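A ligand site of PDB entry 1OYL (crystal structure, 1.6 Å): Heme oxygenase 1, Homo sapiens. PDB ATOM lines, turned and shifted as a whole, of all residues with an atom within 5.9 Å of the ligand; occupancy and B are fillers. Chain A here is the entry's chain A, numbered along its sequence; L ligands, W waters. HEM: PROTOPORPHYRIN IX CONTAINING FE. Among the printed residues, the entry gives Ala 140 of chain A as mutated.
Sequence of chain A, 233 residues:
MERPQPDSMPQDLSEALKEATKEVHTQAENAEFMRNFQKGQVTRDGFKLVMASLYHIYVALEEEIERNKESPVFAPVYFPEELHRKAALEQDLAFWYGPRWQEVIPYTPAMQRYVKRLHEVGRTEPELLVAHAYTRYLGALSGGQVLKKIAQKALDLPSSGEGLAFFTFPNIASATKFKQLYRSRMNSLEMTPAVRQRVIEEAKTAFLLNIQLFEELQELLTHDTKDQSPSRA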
ATOM      1  N   SER A  14       1.980  35.308  -2.465  1.00  0.00           N
ATOM      2  CA  SER A  14       2.297  34.354  -3.520  1.00  0.00           C
ATOM      3  C   SER A  14       3.112  35.034  -4.619  1.00  0.00           C
ATOM      4  O   SER A  14       4.019  34.439  -5.198  1.00  0.00           O
ATOM      5  CB  SER A  14       1.003  33.787  -4.129  1.00  0.00           C
ATOM      6  OG  SER A  14       0.221  34.797  -4.718  1.00  0.00           O
ATOM      7  N   LEU A  17       6.690  35.735  -3.201  1.00  0.00           N
ATOM      8  CA  LEU A  17       7.465  34.496  -3.180  1.00  0.00           C
ATOM      9  C   LEU A  17       8.015  34.115  -4.553  1.00  0.00           C
ATOM     10  O   LEU A  17       9.199  33.805  -4.690  1.00  0.00           O
ATOM     11  CB  LEU A  17       6.607  33.348  -2.639  1.00  0.00           C
ATOM     12  CG  LEU A  17       6.379  33.337  -1.130  1.00  0.00           C
ATOM     13  CD1 LEU A  17       5.292  32.339  -0.779  1.00  0.00           C
ATOM     14  CD2 LEU A  17       7.693  32.992  -0.426  1.00  0.00           C
ATOM     15  N   LYS A  18       7.146  34.142  -5.561  1.00  0.00           N
ATOM     16  CA  LYS A  18       7.561  33.794  -6.913  1.00  0.00           C
ATOM     17  C   LYS A  18       8.689  34.710  -7.383  1.00  0.00           C
ATOM     18  O   LYS A  18       9.670  34.252  -7.971  1.00  0.00           O
ATOM     19  CB  LYS A  18       6.362  33.918  -7.870  1.00  0.00           C
ATOM     20  CG  LYS A  18       6.637  33.402  -9.265  1.00  0.00           C
ATOM     21  CD  LYS A  18       5.388  33.458 -10.137  1.00  0.00           C
ATOM     22  CE  LYS A  18       5.597  32.753 -11.476  1.00  0.00           C
ATOM     23  N   THR A  21      12.116  34.162  -5.359  1.00  0.00           N
ATOM     24  CA  THR A  21      12.788  32.889  -5.583  1.00  0.00           C
ATOM     25  C   THR A  21      13.174  32.593  -7.024  1.00  0.00           C
ATOM     26  O   THR A  21      13.629  31.491  -7.326  1.00  0.00           O
ATOM     27  CB  THR A  21      11.941  31.704  -5.064  1.00  0.00           C
ATOM     28  OG1 THR A  21      10.675  31.697  -5.733  1.00  0.00           O
ATOM     29  CG2 THR A  21      11.729  31.804  -3.567  1.00  0.00           C
ATOM     30  N   HIS A  25      15.576  29.567  -8.021  1.00  0.00           N
ATOM     31  CA  HIS A  25      14.895  28.540  -8.805  1.00  0.00           C
ATOM     32  C   HIS A  25      15.753  28.195 -10.011  1.00  0.00           C
ATOM     33  O   HIS A  25      15.924  27.025 -10.342  1.00  0.00           O
ATOM     34  CB  HIS A  25      13.514  29.018  -9.271  1.00  0.00           C
ATOM     35  CG  HIS A  25      12.731  27.973 -10.005  1.00  0.00           C
ATOM     36  ND1 HIS A  25      13.009  27.621 -11.302  1.00  0.00           N
ATOM     37  CD2 HIS A  25      11.715  27.179  -9.608  1.00  0.00           C
ATOM     38  CE1 HIS A  25      12.202  26.644 -11.673  1.00  0.00           C
ATOM     39  NE2 HIS A  25      11.407  26.358 -10.659  1.00  0.00           N
ATOM     40  N   ALA A  28      18.517  25.993  -9.127  1.00  0.00           N
ATOM     41  CA  ALA A  28      18.096  24.610  -9.003  1.00  0.00           C
ATOM     42  C   ALA A  28      18.035  23.950 -10.374  1.00  0.00           C
ATOM     43  O   ALA A  28      18.423  22.787 -10.527  1.00  0.00           O
ATOM     44  CB  ALA A  28      16.731  24.527  -8.313  1.00  0.00           C
ATOM     45  N   GLU A  29      17.548  24.684 -11.366  1.00  0.00           N
ATOM     46  CA  GLU A  29      17.453  24.149 -12.725  1.00  0.00           C
ATOM     47  C   GLU A  29      18.852  23.899 -13.289  1.00  0.00           C
ATOM     48  O   GLU A  29      19.061  22.992 -14.092  1.00  0.00           O
ATOM     49  CB  GLU A  29      16.744  25.140 -13.655  1.00  0.00           C
ATOM     50  CG  GLU A  29      15.304  25.444 -13.308  1.00  0.00           C
ATOM     51  CD  GLU A  29      14.699  26.461 -14.255  1.00  0.00           C
ATOM     52  OE1 GLU A  29      14.614  26.176 -15.471  1.00  0.00           O
ATOM     53  OE2 GLU A  29      14.319  27.553 -13.777  1.00  0.00           O
ATOM     54  N   MET A  34      20.003  18.081 -11.839  1.00  0.00           N
ATOM     55  CA  MET A  34      18.771  18.501 -12.500  1.00  0.00           C
ATOM     56  C   MET A  34      18.977  18.687 -13.989  1.00  0.00           C
ATOM     57  O   MET A  34      18.057  18.447 -14.780  1.00  0.00           O
ATOM     58  CB  MET A  34      18.232  19.794 -11.880  1.00  0.00           C
ATOM     59  CG  MET A  34      17.498  19.595 -10.571  1.00  0.00           C
ATOM     60  SD  MET A  34      15.989  18.615 -10.735  1.00  0.00           S
ATOM     61  CE  MET A  34      16.606  16.991 -10.401  1.00  0.00           C
ATOM     62  N   PHE A  37      18.960  15.294 -15.504  1.00  0.00           N
ATOM     63  CA  PHE A  37      17.590  14.795 -15.439  1.00  0.00           C
ATOM     64  C   PHE A  37      16.790  15.389 -16.596  1.00  0.00           C
ATOM     65  O   PHE A  37      15.987  14.701 -17.224  1.00  0.00           O
ATOM     66  CB  PHE A  37      16.956  15.158 -14.095  1.00  0.00           C
ATOM     67  CG  PHE A  37      15.595  14.567 -13.874  1.00  0.00           C
ATOM     68  CD1 PHE A  37      14.476  15.086 -14.510  1.00  0.00           C
ATOM     69  CD2 PHE A  37      15.429  13.461 -13.032  1.00  0.00           C
ATOM     70  CE1 PHE A  37      13.210  14.528 -14.314  1.00  0.00           C
ATOM     71  CE2 PHE A  37      14.172  12.896 -12.829  1.00  0.00           C
ATOM     72  CZ  PHE A  37      13.062  13.434 -13.472  1.00  0.00           C
ATOM     73  N   GLN A  38      17.013  16.667 -16.868  1.00  0.00           N
ATOM     74  CA  GLN A  38      16.303  17.358 -17.945  1.00  0.00           C
ATOM     75  C   GLN A  38      16.802  16.898 -19.311  1.00  0.00           C
ATOM     76  O   GLN A  38      16.031  16.817 -20.270  1.00  0.00           O
ATOM     77  CB  GLN A  38      16.497  18.880 -17.815  1.00  0.00           C
ATOM     78  CG  GLN A  38      15.897  19.475 -16.552  1.00  0.00           C
ATOM     79  OE1 GLN A  38      15.762  21.767 -17.226  1.00  0.00           O
ATOM     80  NE2 GLN A  38      16.953  21.303 -15.387  1.00  0.00           N
ATOM     81  N   TYR A 114      17.944  18.859   5.424  1.00  0.00           N
ATOM     82  CA  TYR A 114      16.650  19.350   4.978  1.00  0.00           C
ATOM     83  C   TYR A 114      15.582  18.979   6.014  1.00  0.00           C
ATOM     84  O   TYR A 114      14.792  19.821   6.458  1.00  0.00           O
ATOM     85  CB  TYR A 114      16.310  18.734   3.611  1.00  0.00           C
ATOM     86  CG  TYR A 114      15.277  19.473   2.775  1.00  0.00           C
ATOM     87  CD1 TYR A 114      14.242  20.218   3.354  1.00  0.00           C
ATOM     88  CD2 TYR A 114      15.302  19.357   1.372  1.00  0.00           C
ATOM     89  CE1 TYR A 114      13.272  20.810   2.566  1.00  0.00           C
ATOM     90  CE2 TYR A 114      14.332  19.950   0.584  1.00  0.00           C
ATOM     91  CZ  TYR A 114      13.317  20.681   1.178  1.00  0.00           C
ATOM     92  OH  TYR A 114      12.347  21.265   0.395  1.00  0.00           O
ATOM     93  N   TYR A 134       4.792  25.826   0.288  1.00  0.00           N
ATOM     94  CA  TYR A 134       4.744  26.519  -0.995  1.00  0.00           C
ATOM     95  C   TYR A 134       5.763  25.933  -1.967  1.00  0.00           C
ATOM     96  O   TYR A 134       5.425  25.528  -3.085  1.00  0.00           O
ATOM     97  CB  TYR A 134       5.030  28.016  -0.795  1.00  0.00           C
ATOM     98  CG  TYR A 134       5.497  28.751  -2.043  1.00  0.00           C
ATOM     99  CD1 TYR A 134       4.608  29.101  -3.059  1.00  0.00           C
ATOM    100  CD2 TYR A 134       6.847  29.077  -2.217  1.00  0.00           C
ATOM    101  CE1 TYR A 134       5.047  29.760  -4.221  1.00  0.00           C
ATOM    102  CE2 TYR A 134       7.292  29.734  -3.364  1.00  0.00           C
ATOM    103  CZ  TYR A 134       6.399  30.077  -4.352  1.00  0.00           C
ATOM    104  OH  TYR A 134       6.857  30.713  -5.494  1.00  0.00           O
ATOM    105  N   THR A 135       7.020  25.872  -1.526  1.00  0.00           N
ATOM    106  CA  THR A 135       8.107  25.364  -2.352  1.00  0.00           C
ATOM    107  C   THR A 135       7.885  23.927  -2.822  1.00  0.00           C
ATOM    108  O   THR A 135       8.065  23.623  -3.999  1.00  0.00           O
ATOM    109  CB  THR A 135       9.444  25.448  -1.596  1.00  0.00           C
ATOM    110  OG1 THR A 135       9.698  26.817  -1.221  1.00  0.00           O
ATOM    111  CG2 THR A 135      10.586  24.967  -2.457  1.00  0.00           C
ATOM    112  N   ARG A 136       7.484  23.064  -1.900  1.00  0.00           N
ATOM    113  CA  ARG A 136       7.259  21.666  -2.248  1.00  0.00           C
ATOM    114  C   ARG A 136       5.991  21.414  -3.051  1.00  0.00           C
ATOM    115  O   ARG A 136       6.057  20.862  -4.152  1.00  0.00           O
ATOM    116  CB  ARG A 136       7.267  20.798  -0.982  1.00  0.00           C
ATOM    117  CG  ARG A 136       8.631  20.740  -0.288  1.00  0.00           C
ATOM    118  CD  ARG A 136       9.304  19.382  -0.460  1.00  0.00           C
ATOM    119  NE  ARG A 136       9.488  18.980  -1.857  1.00  0.00           N
ATOM    120  CZ  ARG A 136      10.643  19.033  -2.513  1.00  0.00           C
ATOM    121  NH1 ARG A 136      11.730  19.494  -1.921  1.00  0.00           N
ATOM    122  NH2 ARG A 136      10.706  18.597  -3.771  1.00  0.00           N
ATOM    123  N   LEU A 138       3.510  23.708  -4.406  1.00  0.00           N
ATOM    124  CA  LEU A 138       3.253  24.510  -5.582  1.00  0.00           C
ATOM    125  C   LEU A 138       4.302  24.187  -6.642  1.00  0.00           C
ATOM    126  O   LEU A 138       4.051  24.263  -7.839  1.00  0.00           O
ATOM    127  CB  LEU A 138       3.267  26.006  -5.242  1.00  0.00           C
ATOM    128  CG  LEU A 138       2.346  26.865  -6.113  1.00  0.00           C
ATOM    129  CD1 LEU A 138       0.915  26.358  -6.002  1.00  0.00           C
ATOM    130  CD2 LEU A 138       2.449  28.314  -5.678  1.00  0.00           C
ATOM    131  N   GLY A 139       5.493  23.797  -6.182  1.00  0.00           N
ATOM    132  CA  GLY A 139       6.548  23.438  -7.109  1.00  0.00           C
ATOM    133  C   GLY A 139       6.231  22.135  -7.836  1.00  0.00           C
ATOM    134  O   GLY A 139       6.440  22.031  -9.052  1.00  0.00           O
ATOM    135  N   ALA A 140       5.703  21.169  -7.101  1.00  0.00           N
ATOM    136  CA  ALA A 140       5.349  19.867  -7.672  1.00  0.00           C
ATOM    137  C   ALA A 140       4.155  19.993  -8.605  1.00  0.00           C
ATOM    138  O   ALA A 140       3.980  19.177  -9.518  1.00  0.00           O
ATOM    139  CB  ALA A 140       5.035  18.882  -6.550  1.00  0.00           C
ATOM    140  N   SER A 142       3.626  22.727 -10.428  1.00  0.00           N
ATOM    141  CA  SER A 142       3.990  23.588 -11.543  1.00  0.00           C
ATOM    142  C   SER A 142       4.777  22.876 -12.638  1.00  0.00           C
ATOM    143  O   SER A 142       4.547  23.124 -13.822  1.00  0.00           O
ATOM    144  CB  SER A 142       4.800  24.783 -11.025  1.00  0.00           C
ATOM    145  OG  SER A 142       4.017  25.579 -10.137  1.00  0.00           O
ATOM    146  N   GLY A 143       5.680  21.990 -12.253  1.00  0.00           N
ATOM    147  CA  GLY A 143       6.463  21.275 -13.238  1.00  0.00           C
ATOM    148  C   GLY A 143       6.502  19.767 -13.043  1.00  0.00           C
ATOM    149  O   GLY A 143       7.358  19.093 -13.616  1.00  0.00           O
ATOM    150  N   LEU A 147       8.381  16.474 -15.351  1.00  0.00           N
ATOM    151  CA  LEU A 147       9.277  15.567 -14.653  1.00  0.00           C
ATOM    152  C   LEU A 147       8.842  14.125 -14.875  1.00  0.00           C
ATOM    153  O   LEU A 147       9.650  13.252 -15.197  1.00  0.00           O
ATOM    154  CB  LEU A 147       9.283  15.860 -13.153  1.00  0.00           C
ATOM    155  CG  LEU A 147       9.466  17.316 -12.708  1.00  0.00           C
ATOM    156  CD1 LEU A 147       9.442  17.384 -11.191  1.00  0.00           C
ATOM    157  CD2 LEU A 147      10.773  17.864 -13.248  1.00  0.00           C
ATOM    158  N   LYS A 179      -4.178  25.663  -7.792  1.00  0.00           N
ATOM    159  CA  LYS A 179      -3.088  26.590  -7.530  1.00  0.00           C
ATOM    160  C   LYS A 179      -3.633  27.984  -7.264  1.00  0.00           C
ATOM    161  O   LYS A 179      -3.078  28.745  -6.471  1.00  0.00           O
ATOM    162  CB  LYS A 179      -2.100  26.603  -8.691  1.00  0.00           C
ATOM    163  CG  LYS A 179      -1.207  25.374  -8.734  1.00  0.00           C
ATOM    164  CD  LYS A 179      -0.159  25.446  -9.838  1.00  0.00           C
ATOM    165  CE  LYS A 179      -0.778  25.290 -11.212  1.00  0.00           C
ATOM    166  NZ  LYS A 179       0.259  25.322 -12.284  1.00  0.00           N
ATOM    167  N   ARG A 183      -3.013  29.843  -3.822  1.00  0.00           N
ATOM    168  CA  ARG A 183      -2.409  31.175  -3.805  1.00  0.00           C
ATOM    169  C   ARG A 183      -3.325  32.123  -3.030  1.00  0.00           C
ATOM    170  O   ARG A 183      -2.842  32.934  -2.230  1.00  0.00           O
ATOM    171  CB  ARG A 183      -2.199  31.695  -5.227  1.00  0.00           C
ATOM    172  CG  ARG A 183      -1.103  30.976  -5.996  1.00  0.00           C
ATOM    173  CD  ARG A 183      -0.718  31.759  -7.239  1.00  0.00           C
ATOM    174  NE  ARG A 183       0.457  31.192  -7.916  1.00  0.00           N
ATOM    175  CZ  ARG A 183       0.402  30.278  -8.876  1.00  0.00           C
ATOM    176  NH1 ARG A 183      -0.765  29.806  -9.294  1.00  0.00           N
ATOM    177  NH2 ARG A 183       1.518  29.824  -9.422  1.00  0.00           N
ATOM    178  N   ALA A 206      14.696  27.035   1.384  1.00  0.00           N
ATOM    179  CA  ALA A 206      14.189  25.741   0.928  1.00  0.00           C
ATOM    180  C   ALA A 206      14.878  25.359  -0.373  1.00  0.00           C
ATOM    181  O   ALA A 206      15.355  24.230  -0.530  1.00  0.00           O
ATOM    182  CB  ALA A 206      12.686  25.807   0.731  1.00  0.00           C
ATOM    183  N   PHE A 207      14.930  26.285  -1.315  1.00  0.00           N
ATOM    184  CA  PHE A 207      15.584  26.006  -2.581  1.00  0.00           C
ATOM    185  C   PHE A 207      17.040  25.623  -2.365  1.00  0.00           C
ATOM    186  O   PHE A 207      17.549  24.673  -2.959  1.00  0.00           O
ATOM    187  CB  PHE A 207      15.503  27.203  -3.536  1.00  0.00           C
ATOM    188  CG  PHE A 207      14.212  27.292  -4.297  1.00  0.00           C
ATOM    189  CD1 PHE A 207      13.089  27.896  -3.734  1.00  0.00           C
ATOM    190  CD2 PHE A 207      14.128  26.778  -5.581  1.00  0.00           C
ATOM    191  CE1 PHE A 207      11.904  27.985  -4.459  1.00  0.00           C
ATOM    192  CE2 PHE A 207      12.946  26.862  -6.314  1.00  0.00           C
ATOM    193  CZ  PHE A 207      11.833  27.468  -5.749  1.00  0.00           C
ATOM    194  N   ASN A 210      17.482  22.154  -1.268  1.00  0.00           N
ATOM    195  CA  ASN A 210      17.278  21.237  -2.385  1.00  0.00           C
ATOM    196  C   ASN A 210      18.545  21.195  -3.238  1.00  0.00           C
ATOM    197  O   ASN A 210      18.987  20.123  -3.684  1.00  0.00           O
ATOM    198  CB  ASN A 210      16.109  21.695  -3.254  1.00  0.00           C
ATOM    199  CG  ASN A 210      14.774  21.243  -2.708  1.00  0.00           C
ATOM    200  OD1 ASN A 210      14.359  20.106  -2.912  1.00  0.00           O
ATOM    201  ND2 ASN A 210      14.075  22.140  -2.024  1.00  0.00           N
ATOM    202  N   PHE A 214      20.859  18.063  -4.274  1.00  0.00           N
ATOM    203  CA  PHE A 214      21.183  17.648  -5.639  1.00  0.00           C
ATOM    204  C   PHE A 214      22.684  17.470  -5.799  1.00  0.00           C
ATOM    205  O   PHE A 214      23.134  16.520  -6.449  1.00  0.00           O
ATOM    206  CB  PHE A 214      20.720  18.685  -6.673  1.00  0.00           C
ATOM    207  CG  PHE A 214      19.226  18.866  -6.719  1.00  0.00           C
ATOM    208  CD1 PHE A 214      18.361  17.826  -6.402  1.00  0.00           C
ATOM    209  CD2 PHE A 214      18.696  20.093  -7.112  1.00  0.00           C
ATOM    210  CE1 PHE A 214      16.982  17.988  -6.483  1.00  0.00           C
ATOM    211  CE2 PHE A 214      17.314  20.276  -7.195  1.00  0.00           C
ATOM    212  CZ  PHE A 214      16.462  19.225  -6.880  1.00  0.00           C
HETATM  213  CHA HEM L   1       7.512  26.928 -10.885  1.00  0.00           C
HETATM  214  CHB HEM L   1      10.244  24.290 -13.948  1.00  0.00           C
HETATM  215  CHC HEM L   1      12.896  22.725 -10.148  1.00  0.00           C
HETATM  216  CHD HEM L   1       9.827  24.962  -7.100  1.00  0.00           C
HETATM  217  C1A HEM L   1       8.076  26.389 -12.036  1.00  0.00           C
HETATM  218  C2A HEM L   1       7.679  26.756 -13.384  1.00  0.00           C
HETATM  219  C3A HEM L   1       8.334  25.932 -14.236  1.00  0.00           C
HETATM  220  C4A HEM L   1       9.248  25.130 -13.425  1.00  0.00           C
HETATM  221  CMA HEM L   1       8.089  25.842 -15.744  1.00  0.00           C
HETATM  222  CAA HEM L   1       6.820  27.965 -13.779  1.00  0.00           C
HETATM  223  CBA HEM L   1       5.348  27.644 -13.842  1.00  0.00           C
HETATM  224  CGA HEM L   1       4.507  28.860 -14.187  1.00  0.00           C
HETATM  225  O1A HEM L   1       4.454  29.795 -13.360  1.00  0.00           O
HETATM  226  O2A HEM L   1       3.918  28.885 -15.283  1.00  0.00           O
HETATM  227  C1B HEM L   1      11.210  23.643 -13.153  1.00  0.00           C
HETATM  228  C2B HEM L   1      12.332  22.886 -13.697  1.00  0.00           C
HETATM  229  C3B HEM L   1      13.104  22.495 -12.647  1.00  0.00           C
HETATM  230  C4B HEM L   1      12.441  22.977 -11.434  1.00  0.00           C
HETATM  231  CMB HEM L   1      12.635  22.655 -15.181  1.00  0.00           C
HETATM  232  CAB HEM L   1      14.326  21.827 -12.701  1.00  0.00           C
HETATM  233  CBB HEM L   1      14.460  20.482 -13.242  1.00  0.00           C
HETATM  234  C1C HEM L   1      12.268  23.197  -8.990  1.00  0.00           C
HETATM  235  C2C HEM L   1      12.707  22.882  -7.634  1.00  0.00           C
HETATM  236  C3C HEM L   1      11.810  23.469  -6.780  1.00  0.00           C
HETATM  237  C4C HEM L   1      10.845  24.162  -7.615  1.00  0.00           C
HETATM  238  CMC HEM L   1      13.941  22.073  -7.247  1.00  0.00           C
HETATM  239  CAC HEM L   1      11.840  23.492  -5.377  1.00  0.00           C
HETATM  240  CBC HEM L   1      12.065  22.327  -4.527  1.00  0.00           C
HETATM  241  C1D HEM L   1       8.969  25.697  -7.888  1.00  0.00           C
HETATM  242  C2D HEM L   1       7.972  26.576  -7.340  1.00  0.00           C
HETATM  243  C3D HEM L   1       7.291  27.085  -8.370  1.00  0.00           C
HETATM  244  C4D HEM L   1       7.897  26.585  -9.592  1.00  0.00           C
HETATM  245  CMD HEM L   1       7.698  26.828  -5.859  1.00  0.00           C
HETATM  246  CAD HEM L   1       6.068  27.969  -8.192  1.00  0.00           C
HETATM  247  CBD HEM L   1       6.304  29.347  -8.762  1.00  0.00           C
HETATM  248  CGD HEM L   1       5.114  30.255  -8.564  1.00  0.00           C
HETATM  249  O1D HEM L   1       4.881  30.680  -7.416  1.00  0.00           O
HETATM  250  O2D HEM L   1       4.407  30.534  -9.548  1.00  0.00           O
HETATM  251  NA  HEM L   1       9.078  25.422 -12.056  1.00  0.00           N
HETATM  252  NB  HEM L   1      11.297  23.718 -11.762  1.00  0.00           N
HETATM  253  NC  HEM L   1      11.109  23.992  -8.979  1.00  0.00           N
HETATM  254  ND  HEM L   1       8.930  25.705  -9.277  1.00  0.00           N
HETATM  255 FE   HEM L   1      10.087  24.721 -10.522  1.00  0.00          FE
HETATM  256  O   HOH W   1       3.010  32.316  -6.716  1.00  0.00           O
HETATM  257  O   HOH W   2       8.828  23.264 -10.631  1.00  0.00           O
HETATM  258  O   HOH W   3      12.597  19.231 -15.168  1.00  0.00           O
HETATM  259  O   HOH W   4      10.140  20.569  -7.478  1.00  0.00           O
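O2D of the ligand is in salt-bridge range of NH2 of Arg 183 (3.0 Å).
The side-chain hydroxyl (OH) of Tyr 134 lies within hydrogen-bond range of an oxygen (O1D) of the ligand, 2.8 Å away.
FE of the ligand is bound by NE2 of His 25 (2.1 Å).
The backbone carbonyl oxygen of Glu 29 sits at hydrogen-bond distance from the side-chain amide nitrogen of Gln 38 (3.0 Å).
The side-chain amide oxygen (OD1) of Asn 210 lies within hydrogen-bond range of the guanidinium group (NH1) of Arg 136, at 2.9 Å.
O of Ala 206 is in hydrogen-bond range of ND2 of Asn 210 (2.9 Å).
NE2 of Gln 38 sits close to O of Met 34, 3.1 Å away.
The guanidinium group (NH1) of Arg 136 sits at hydrogen-bond distance from the side-chain hydroxyl (OH) of Tyr 114, 3.0 Å away.
The side-chain hydroxyl of Ser 142 is in hydrogen-bond range of the backbone carbonyl oxygen of Leu 138, at 2.6 Å.
OE2 of Glu 29 sits at hydrogen-bond distance from ND1 of His 25 (2.8 Å).
The backbone NH (N) of Lys 18 lies within hydrogen-bond range of the side-chain hydroxyl (OH) of Tyr 134 (3.4 Å).
Merely in contact with the ligand: Lys 18 (3.1 Å), Asn 210 (3.2 Å), Gln 38 (3.4 Å), Gly 139 (3.4 Å), Ser 142 (3.5 Å), Met 34 (3.5 Å), Phe 207 (3.5 Å), Thr 135 (3.5 Å), Glu 29 (3.7 Å), Leu 138 (3.8 Å), Phe 214 (3.8 Å), Arg 136 (3.9 Å) and Ala 28 (3.9 Å).
Hydrophobic or aromatic side chains within 4 Å of the ligand: His 25, Ala 28, Met 34, Tyr 134, Leu 138, Phe 207 and Phe 214.
Within 4 Å of the ligand: Lys 18, His 25, Ala 28, Glu 29, Met 34, Gln 38, Tyr 134, Thr 135, Arg 136, Leu 138, Gly 139, Ser 142, Arg 183, Phe 207, Asn 210 and Phe 214.
The nearest printed residue that does not touch the ligand is Ser 14 (4.4 Å).
Water W1 lies within hydrogen-bond range of an oxygen (O1D) of the ligand (2.6 Å), the backbone carbonyl oxygen (O) of Ser 14 (2.8 Å) and the guanidinium group (NE) of Arg 183 (3.0 Å).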
